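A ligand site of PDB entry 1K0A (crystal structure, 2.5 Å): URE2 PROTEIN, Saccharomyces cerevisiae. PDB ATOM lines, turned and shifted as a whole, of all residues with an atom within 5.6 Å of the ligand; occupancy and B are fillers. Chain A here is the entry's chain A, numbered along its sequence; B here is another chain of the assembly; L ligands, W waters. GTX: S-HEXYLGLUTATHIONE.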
ATOM      1  N   HIS A  25      18.746  -2.276  13.247  1.00  0.00           N
ATOM      2  CA  HIS A  25      20.131  -2.035  13.588  1.00  0.00           C
ATOM      3  C   HIS A  25      20.973  -3.187  13.020  1.00  0.00           C
ATOM      4  O   HIS A  25      20.511  -4.325  12.953  1.00  0.00           O
ATOM      5  CB  HIS A  25      20.331  -1.948  15.089  1.00  0.00           C
ATOM      6  CG  HIS A  25      21.685  -1.466  15.465  1.00  0.00           C
ATOM      7  ND1 HIS A  25      21.930  -0.165  15.835  1.00  0.00           N
ATOM      8  CD2 HIS A  25      22.894  -2.090  15.454  1.00  0.00           C
ATOM      9  CE1 HIS A  25      23.233   0.004  16.027  1.00  0.00           C
ATOM     10  NE2 HIS A  25      23.836  -1.147  15.796  1.00  0.00           N
ATOM     11  N   SER A  27      23.309  -4.745  14.298  1.00  0.00           N
ATOM     12  CA  SER A  27      23.592  -5.748  15.324  1.00  0.00           C
ATOM     13  C   SER A  27      22.328  -6.131  16.086  1.00  0.00           C
ATOM     14  O   SER A  27      22.388  -6.597  17.228  1.00  0.00           O
ATOM     15  CB  SER A  27      24.631  -5.200  16.311  1.00  0.00           C
ATOM     16  OG  SER A  27      25.816  -4.796  15.648  1.00  0.00           O
ATOM     17  N   ALA A  28      21.175  -5.936  15.453  1.00  0.00           N
ATOM     18  CA  ALA A  28      19.899  -6.243  16.080  1.00  0.00           C
ATOM     19  C   ALA A  28      19.276  -7.495  15.497  1.00  0.00           C
ATOM     20  O   ALA A  28      18.621  -7.442  14.463  1.00  0.00           O
ATOM     21  CB  ALA A  28      18.944  -5.064  15.925  1.00  0.00           C
ATOM     22  N   PRO A  29      19.475  -8.648  16.156  1.00  0.00           N
ATOM     23  CA  PRO A  29      18.878  -9.880  15.620  1.00  0.00           C
ATOM     24  C   PRO A  29      17.373  -9.685  15.469  1.00  0.00           C
ATOM     25  O   PRO A  29      16.786 -10.071  14.453  1.00  0.00           O
ATOM     26  CB  PRO A  29      19.241 -10.922  16.671  1.00  0.00           C
ATOM     27  CG  PRO A  29      20.545 -10.400  17.232  1.00  0.00           C
ATOM     28  CD  PRO A  29      20.251  -8.926  17.375  1.00  0.00           C
ATOM     29  N   ASN A  30      16.755  -9.076  16.483  1.00  0.00           N
ATOM     30  CA  ASN A  30      15.320  -8.817  16.485  1.00  0.00           C
ATOM     31  C   ASN A  30      14.929  -8.079  15.226  1.00  0.00           C
ATOM     32  O   ASN A  30      13.866  -8.327  14.654  1.00  0.00           O
ATOM     33  CB  ASN A  30      14.942  -7.989  17.714  1.00  0.00           C
ATOM     34  CG  ASN A  30      14.731  -8.842  18.949  1.00  0.00           C
ATOM     35  OD1 ASN A  30      15.077  -8.444  20.062  1.00  0.00           O
ATOM     36  ND2 ASN A  30      14.131 -10.022  18.773  1.00  0.00           N
ATOM     37  N   GLY A  31      15.797  -7.181  14.774  1.00  0.00           N
ATOM     38  CA  GLY A  31      15.526  -6.444  13.556  1.00  0.00           C
ATOM     39  C   GLY A  31      15.612  -7.346  12.327  1.00  0.00           C
ATOM     40  O   GLY A  31      14.790  -7.254  11.414  1.00  0.00           O
ATOM     41  N   LYS A  33      15.044 -10.403  12.294  1.00  0.00           N
ATOM     42  CA  LYS A  33      13.942 -11.344  12.397  1.00  0.00           C
ATOM     43  C   LYS A  33      12.804 -10.831  11.506  1.00  0.00           C
ATOM     44  O   LYS A  33      12.218 -11.588  10.725  1.00  0.00           O
ATOM     45  CB  LYS A  33      13.492 -11.424  13.861  1.00  0.00           C
ATOM     46  CG  LYS A  33      12.564 -12.585  14.177  1.00  0.00           C
ATOM     47  CD  LYS A  33      12.280 -12.683  15.692  1.00  0.00           C
ATOM     48  CE  LYS A  33      11.273 -11.637  16.126  1.00  0.00           C
ATOM     49  NZ  LYS A  33      10.791 -11.851  17.525  1.00  0.00           N
ATOM     50  N   PHE A  52      22.047   5.085  17.364  1.00  0.00           N
ATOM     51  CA  PHE A  52      21.717   5.575  18.696  1.00  0.00           C
ATOM     52  C   PHE A  52      22.757   6.530  19.248  1.00  0.00           C
ATOM     53  O   PHE A  52      22.435   7.421  20.034  1.00  0.00           O
ATOM     54  CB  PHE A  52      21.508   4.389  19.647  1.00  0.00           C
ATOM     55  CG  PHE A  52      20.314   3.526  19.287  1.00  0.00           C
ATOM     56  CD1 PHE A  52      20.344   2.717  18.148  1.00  0.00           C
ATOM     57  CD2 PHE A  52      19.174   3.534  20.077  1.00  0.00           C
ATOM     58  CE1 PHE A  52      19.237   1.940  17.801  1.00  0.00           C
ATOM     59  CE2 PHE A  52      18.060   2.760  19.741  1.00  0.00           C
ATOM     60  CZ  PHE A  52      18.089   1.964  18.596  1.00  0.00           C
ATOM     61  N   ALA A  69      11.222   3.497  21.873  1.00  0.00           N
ATOM     62  CA  ALA A  69      12.493   3.995  21.362  1.00  0.00           C
ATOM     63  C   ALA A  69      13.522   2.903  21.095  1.00  0.00           C
ATOM     64  O   ALA A  69      14.726   3.127  21.225  1.00  0.00           O
ATOM     65  CB  ALA A  69      13.063   5.028  22.339  1.00  0.00           C
ATOM     66  N   ARG A  70      13.053   1.713  20.725  1.00  0.00           N
ATOM     67  CA  ARG A  70      13.921   0.590  20.419  1.00  0.00           C
ATOM     68  C   ARG A  70      13.584   0.069  19.033  1.00  0.00           C
ATOM     69  O   ARG A  70      12.540   0.412  18.468  1.00  0.00           O
ATOM     70  CB  ARG A  70      13.727  -0.543  21.443  1.00  0.00           C
ATOM     71  CG  ARG A  70      14.619  -0.460  22.695  1.00  0.00           C
ATOM     72  CD  ARG A  70      14.708   0.965  23.224  1.00  0.00           C
ATOM     73  NE  ARG A  70      15.536   1.093  24.423  1.00  0.00           N
ATOM     74  CZ  ARG A  70      15.949   2.260  24.916  1.00  0.00           C
ATOM     75  NH1 ARG A  70      15.626   3.404  24.308  1.00  0.00           N
ATOM     76  NH2 ARG A  70      16.682   2.292  26.019  1.00  0.00           N
ATOM     77  N   VAL A  71      14.461  -0.752  18.470  1.00  0.00           N
ATOM     78  CA  VAL A  71      14.207  -1.339  17.157  1.00  0.00           C
ATOM     79  C   VAL A  71      13.978  -2.820  17.406  1.00  0.00           C
ATOM     80  O   VAL A  71      14.454  -3.378  18.397  1.00  0.00           O
ATOM     81  CB  VAL A  71      15.390  -1.138  16.195  1.00  0.00           C
ATOM     82  CG1 VAL A  71      15.551   0.331  15.885  1.00  0.00           C
ATOM     83  CG2 VAL A  71      16.677  -1.721  16.794  1.00  0.00           C
ATOM     84  N   PRO A  72      13.245  -3.499  16.492  1.00  0.00           N
ATOM     85  CA  PRO A  72      12.633  -2.987  15.268  1.00  0.00           C
ATOM     86  C   PRO A  72      11.269  -2.323  15.418  1.00  0.00           C
ATOM     87  O   PRO A  72      10.569  -2.518  16.412  1.00  0.00           O
ATOM     88  CB  PRO A  72      12.536  -4.219  14.401  1.00  0.00           C
ATOM     89  CG  PRO A  72      12.166  -5.260  15.411  1.00  0.00           C
ATOM     90  CD  PRO A  72      13.150  -4.972  16.535  1.00  0.00           C
ATOM     91  N   TRP A  85       5.349  -1.683  16.734  1.00  0.00           N
ATOM     92  CA  TRP A  85       6.630  -1.844  17.418  1.00  0.00           C
ATOM     93  C   TRP A  85       6.614  -3.220  18.042  1.00  0.00           C
ATOM     94  O   TRP A  85       5.575  -3.872  18.041  1.00  0.00           O
ATOM     95  CB  TRP A  85       6.856  -0.738  18.469  1.00  0.00           C
ATOM     96  CG  TRP A  85       5.661  -0.368  19.278  1.00  0.00           C
ATOM     97  CD1 TRP A  85       4.512   0.201  18.818  1.00  0.00           C
ATOM     98  CD2 TRP A  85       5.501  -0.522  20.693  1.00  0.00           C
ATOM     99  NE1 TRP A  85       3.637   0.408  19.850  1.00  0.00           N
ATOM    100  CE2 TRP A  85       4.212  -0.022  21.018  1.00  0.00           C
ATOM    101  CE3 TRP A  85       6.304  -1.023  21.714  1.00  0.00           C
ATOM    102  CZ2 TRP A  85       3.707  -0.020  22.331  1.00  0.00           C
ATOM    103  CZ3 TRP A  85       5.809  -1.018  23.033  1.00  0.00           C
ATOM    104  CH2 TRP A  85       4.517  -0.517  23.320  1.00  0.00           C
ATOM    105  N   GLU A  86       7.762  -3.652  18.577  1.00  0.00           N
ATOM    106  CA  GLU A  86       7.922  -4.993  19.150  1.00  0.00           C
ATOM    107  C   GLU A  86       7.917  -6.011  17.989  1.00  0.00           C
ATOM    108  O   GLU A  86       6.926  -6.161  17.271  1.00  0.00           O
ATOM    109  CB  GLU A  86       6.811  -5.326  20.156  1.00  0.00           C
ATOM    110  CG  GLU A  86       7.004  -4.682  21.522  1.00  0.00           C
ATOM    111  CD  GLU A  86       8.245  -5.197  22.262  1.00  0.00           C
ATOM    112  OE1 GLU A  86       8.976  -4.359  22.845  1.00  0.00           O
ATOM    113  OE2 GLU A  86       8.498  -6.423  22.289  1.00  0.00           O
ATOM    114  N   SER A  87       9.048  -6.701  17.820  1.00  0.00           N
ATOM    115  CA  SER A  87       9.238  -7.691  16.760  1.00  0.00           C
ATOM    116  C   SER A  87       8.132  -8.749  16.686  1.00  0.00           C
ATOM    117  O   SER A  87       7.713  -9.142  15.593  1.00  0.00           O
ATOM    118  CB  SER A  87      10.607  -8.386  16.915  1.00  0.00           C
ATOM    119  OG  SER A  87      10.658  -9.241  18.056  1.00  0.00           O
ATOM    120  N   GLY A  88       7.672  -9.209  17.847  1.00  0.00           N
ATOM    121  CA  GLY A  88       6.618 -10.200  17.895  1.00  0.00           C
ATOM    122  C   GLY A  88       5.280  -9.687  17.395  1.00  0.00           C
ATOM    123  O   GLY A  88       4.510 -10.434  16.795  1.00  0.00           O
ATOM    124  N   THR A 126      10.741 -14.448  22.118  1.00  0.00           N
ATOM    125  CA  THR A 126      10.914 -13.028  22.411  1.00  0.00           C
ATOM    126  C   THR A 126      10.993 -12.643  23.890  1.00  0.00           C
ATOM    127  O   THR A 126      11.496 -11.560  24.215  1.00  0.00           O
ATOM    128  CB  THR A 126       9.789 -12.171  21.792  1.00  0.00           C
ATOM    129  OG1 THR A 126       8.555 -12.466  22.445  1.00  0.00           O
ATOM    130  CG2 THR A 126       9.661 -12.448  20.303  1.00  0.00           C
ATOM    131  N   GLY A 134      20.496 -11.582  25.675  1.00  0.00           N
ATOM    132  CA  GLY A 134      20.916 -10.197  25.813  1.00  0.00           C
ATOM    133  C   GLY A 134      21.564  -9.875  27.139  1.00  0.00           C
ATOM    134  O   GLY A 134      22.452  -9.032  27.218  1.00  0.00           O
ATOM    135  N   LEU A 137      25.162 -11.301  27.157  1.00  0.00           N
ATOM    136  CA  LEU A 137      26.089 -10.455  26.432  1.00  0.00           C
ATOM    137  C   LEU A 137      26.420  -9.224  27.231  1.00  0.00           C
ATOM    138  O   LEU A 137      27.579  -8.804  27.302  1.00  0.00           O
ATOM    139  CB  LEU A 137      25.516 -10.021  25.082  1.00  0.00           C
ATOM    140  CG  LEU A 137      25.415 -11.068  23.973  1.00  0.00           C
ATOM    141  CD1 LEU A 137      24.663 -10.492  22.771  1.00  0.00           C
ATOM    142  CD2 LEU A 137      26.802 -11.508  23.578  1.00  0.00           C
ATOM    143  N   TRP A 222      19.038 -15.070  16.433  1.00  0.00           N
ATOM    144  CA  TRP A 222      19.702 -15.215  17.715  1.00  0.00           C
ATOM    145  C   TRP A 222      20.667 -16.406  17.781  1.00  0.00           C
ATOM    146  O   TRP A 222      21.714 -16.323  18.438  1.00  0.00           O
ATOM    147  CB  TRP A 222      18.669 -15.282  18.842  1.00  0.00           C
ATOM    148  CG  TRP A 222      17.895 -13.988  18.990  1.00  0.00           C
ATOM    149  CD1 TRP A 222      16.733 -13.647  18.361  1.00  0.00           C
ATOM    150  CD2 TRP A 222      18.273 -12.858  19.778  1.00  0.00           C
ATOM    151  NE1 TRP A 222      16.364 -12.371  18.703  1.00  0.00           N
ATOM    152  CE2 TRP A 222      17.289 -11.851  19.574  1.00  0.00           C
ATOM    153  CE3 TRP A 222      19.347 -12.573  20.633  1.00  0.00           C
ATOM    154  CZ2 TRP A 222      17.346 -10.602  20.200  1.00  0.00           C
ATOM    155  CZ3 TRP A 222      19.404 -11.324  21.259  1.00  0.00           C
ATOM    156  CH2 TRP A 222      18.407 -10.350  21.032  1.00  0.00           C
ATOM    157  N   VAL A 225      24.356 -15.618  17.151  1.00  0.00           N
ATOM    158  CA  VAL A 225      25.166 -14.815  18.056  1.00  0.00           C
ATOM    159  C   VAL A 225      25.421 -15.517  19.385  1.00  0.00           C
ATOM    160  O   VAL A 225      26.225 -15.041  20.179  1.00  0.00           O
ATOM    161  CB  VAL A 225      24.511 -13.437  18.366  1.00  0.00           C
ATOM    162  CG1 VAL A 225      24.035 -12.780  17.087  1.00  0.00           C
ATOM    163  CG2 VAL A 225      23.361 -13.609  19.358  1.00  0.00           C
ATOM    164  N   PHE B 123       3.464  -7.647  23.961  1.00  0.00           N
ATOM    165  CA  PHE B 123       4.803  -8.170  23.805  1.00  0.00           C
ATOM    166  C   PHE B 123       5.798  -7.376  24.628  1.00  0.00           C
ATOM    167  O   PHE B 123       6.766  -7.919  25.157  1.00  0.00           O
ATOM    168  CB  PHE B 123       5.230  -8.155  22.332  1.00  0.00           C
ATOM    169  CG  PHE B 123       4.950  -9.450  21.619  1.00  0.00           C
ATOM    170  CD1 PHE B 123       3.787  -9.618  20.875  1.00  0.00           C
ATOM    171  CD2 PHE B 123       5.857 -10.510  21.697  1.00  0.00           C
ATOM    172  CE1 PHE B 123       3.524 -10.843  20.221  1.00  0.00           C
ATOM    173  CE2 PHE B 123       5.602 -11.732  21.047  1.00  0.00           C
ATOM    174  CZ  PHE B 123       4.435 -11.892  20.307  1.00  0.00           C
ATOM    175  N   SER B 127       7.967  -9.114  27.525  1.00  0.00           N
ATOM    176  CA  SER B 127       9.380  -9.231  27.212  1.00  0.00           C
ATOM    177  C   SER B 127      10.247  -8.070  27.693  1.00  0.00           C
ATOM    178  O   SER B 127      11.472  -8.198  27.757  1.00  0.00           O
ATOM    179  CB  SER B 127       9.584  -9.422  25.709  1.00  0.00           C
ATOM    180  OG  SER B 127       9.483  -8.190  25.028  1.00  0.00           O
ATOM    181  N   GLY B 128       9.642  -6.948  28.041  1.00  0.00           N
ATOM    182  CA  GLY B 128      10.447  -5.827  28.484  1.00  0.00           C
ATOM    183  C   GLY B 128      10.054  -5.267  29.827  1.00  0.00           C
ATOM    184  O   GLY B 128      10.622  -4.286  30.271  1.00  0.00           O
HETATM  185  N1  GTX L   1      11.138  -6.723  22.920  1.00  0.00           N
HETATM  186  CA1 GTX L   1      11.796  -5.962  21.745  1.00  0.00           C
HETATM  187  C1  GTX L   1      11.399  -6.652  20.459  1.00  0.00           C
HETATM  188  O11 GTX L   1      11.207  -5.958  19.448  1.00  0.00           O
HETATM  189  O12 GTX L   1      11.246  -8.025  20.470  1.00  0.00           O
HETATM  190  CB1 GTX L   1      13.346  -5.940  21.976  1.00  0.00           C
HETATM  191  CG1 GTX L   1      14.133  -5.191  20.851  1.00  0.00           C
HETATM  192  CD1 GTX L   1      15.537  -4.900  21.278  1.00  0.00           C
HETATM  193  OE1 GTX L   1      16.051  -5.438  22.297  1.00  0.00           O
HETATM  194  N2  GTX L   1      16.182  -4.039  20.474  1.00  0.00           N
HETATM  195  CA2 GTX L   1      17.569  -3.651  20.763  1.00  0.00           C
HETATM  196  C2  GTX L   1      17.676  -2.061  20.803  1.00  0.00           C
HETATM  197  O2  GTX L   1      16.970  -1.373  20.090  1.00  0.00           O
HETATM  198  CB2 GTX L   1      18.539  -4.108  19.610  1.00  0.00           C
HETATM  199  SG2 GTX L   1      18.570  -5.904  19.379  1.00  0.00           S
HETATM  200  C1S GTX L   1      18.916  -6.653  21.017  1.00  0.00           C
HETATM  201  C2S GTX L   1      20.288  -6.262  21.547  1.00  0.00           C
HETATM  202  C3S GTX L   1      20.979  -7.321  22.402  1.00  0.00           C
HETATM  203  C4S GTX L   1      22.476  -7.646  22.169  1.00  0.00           C
HETATM  204  C5S GTX L   1      22.899  -8.003  20.720  1.00  0.00           C
HETATM  205  C6S GTX L   1      22.366  -9.337  20.167  1.00  0.00           C
HETATM  206  N3  GTX L   1      18.521  -1.534  21.644  1.00  0.00           N
HETATM  207  CA3 GTX L   1      18.149  -1.120  23.001  1.00  0.00           C
HETATM  208  C3  GTX L   1      18.707   0.224  23.288  1.00  0.00           C
HETATM  209  O31 GTX L   1      18.563   0.851  24.385  1.00  0.00           O
HETATM  210  O32 GTX L   1      19.413   0.732  22.275  1.00  0.00           O
HETATM  211  O   HOH W   1      10.940  -3.517  19.087  1.00  0.00           O
HETATM  212  O   HOH W   2       8.375  -8.712  20.413  1.00  0.00           O
HETATM  213  O   HOH W   3      15.151  -3.301  24.165  1.00  0.00           O
HETATM  214  O   HOH W   4      13.064  -7.390  25.130  1.00  0.00           O
HETATM  215  O   HOH W   5      15.472  -8.313  23.970  1.00  0.00           O
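Water W1 lies within hydrogen-bond range of O11 of the ligand, O of Pro 72 and N of Glu 86.
Water W2 lies within hydrogen-bond range of the backbone NH (N) of Gly 88 (2.7 Å), an oxygen (O12) of the ligand (3.0 Å), the side-chain carboxylate (OE2) of Glu 86 (3.0 Å) and the side-chain hydroxyl (OG) of Ser 87 (3.3 Å).
Water W4 bridges N1 of the ligand and O of Ser 127 of chain B.
Merely in contact with the ligand: Asn 30 (3.5 Å), Phe 52 (3.5 Å), Pro 29 (3.5 Å), Ala 28 (3.6 Å), Pro 72 (3.6 Å), Leu 137 (3.6 Å), Trp 222 (3.7 Å) and Ser 27 (3.8 Å).
Hydrophobic or aromatic side chains within 4 Å of the ligand: Ala 28, Pro 29, Phe 52, Val 71, Pro 72, Leu 137 and Trp 222.
13 residues have an atom within 4 Å of the ligand: Ser 27, Ala 28, Pro 29, Asn 30, Phe 52, Arg 70, Val 71, Pro 72, Glu 86, Ser 87, Leu 137, Trp 222 and Ser 127 of chain B.
The nearest printed residue that does not touch the ligand is Val 225 (4.5 Å).
The side-chain hydroxyl of Ser 127 of chain B sits at hydrogen-bond distance from the side-chain carboxylate of Glu 86.
The side-chain hydroxyl of Ser 87 sits at hydrogen-bond distance from the side-chain amino group of Lys 33 (2.7 Å).
The backbone carbonyl oxygen of Phe 123 of chain B sits at hydrogen-bond distance from the side-chain hydroxyl of Ser 127 of chain B, at 2.7 Å.
The indole nitrogen (NE1) of Trp 222 sits close to the side-chain amide nitrogen (ND2) of Asn 30 (3.2 Å).
N1 of the ligand is in salt-bridge range of OE2 of Glu 86, 2.7 Å away.
An oxygen (O11) of the ligand lies within hydrogen-bond range of the backbone NH (N) of Ser 87 (2.8 Å).
O12 of the ligand sits at hydrogen-bond distance from OG of Ser 87, 2.8 Å away.
O2 of the ligand lies within hydrogen-bond range of N of Val 71 (3.1 Å).
O of Val 71 lies within hydrogen-bond range of N2 of the ligand, 2.8 Å away.
NH2 of Arg 70 lies within salt-bridge range of O31 of the ligand, at 2.9 Å.
OG of Ser 127 of chain B sits at hydrogen-bond distance from N1 of the ligand, 3.1 Å away.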
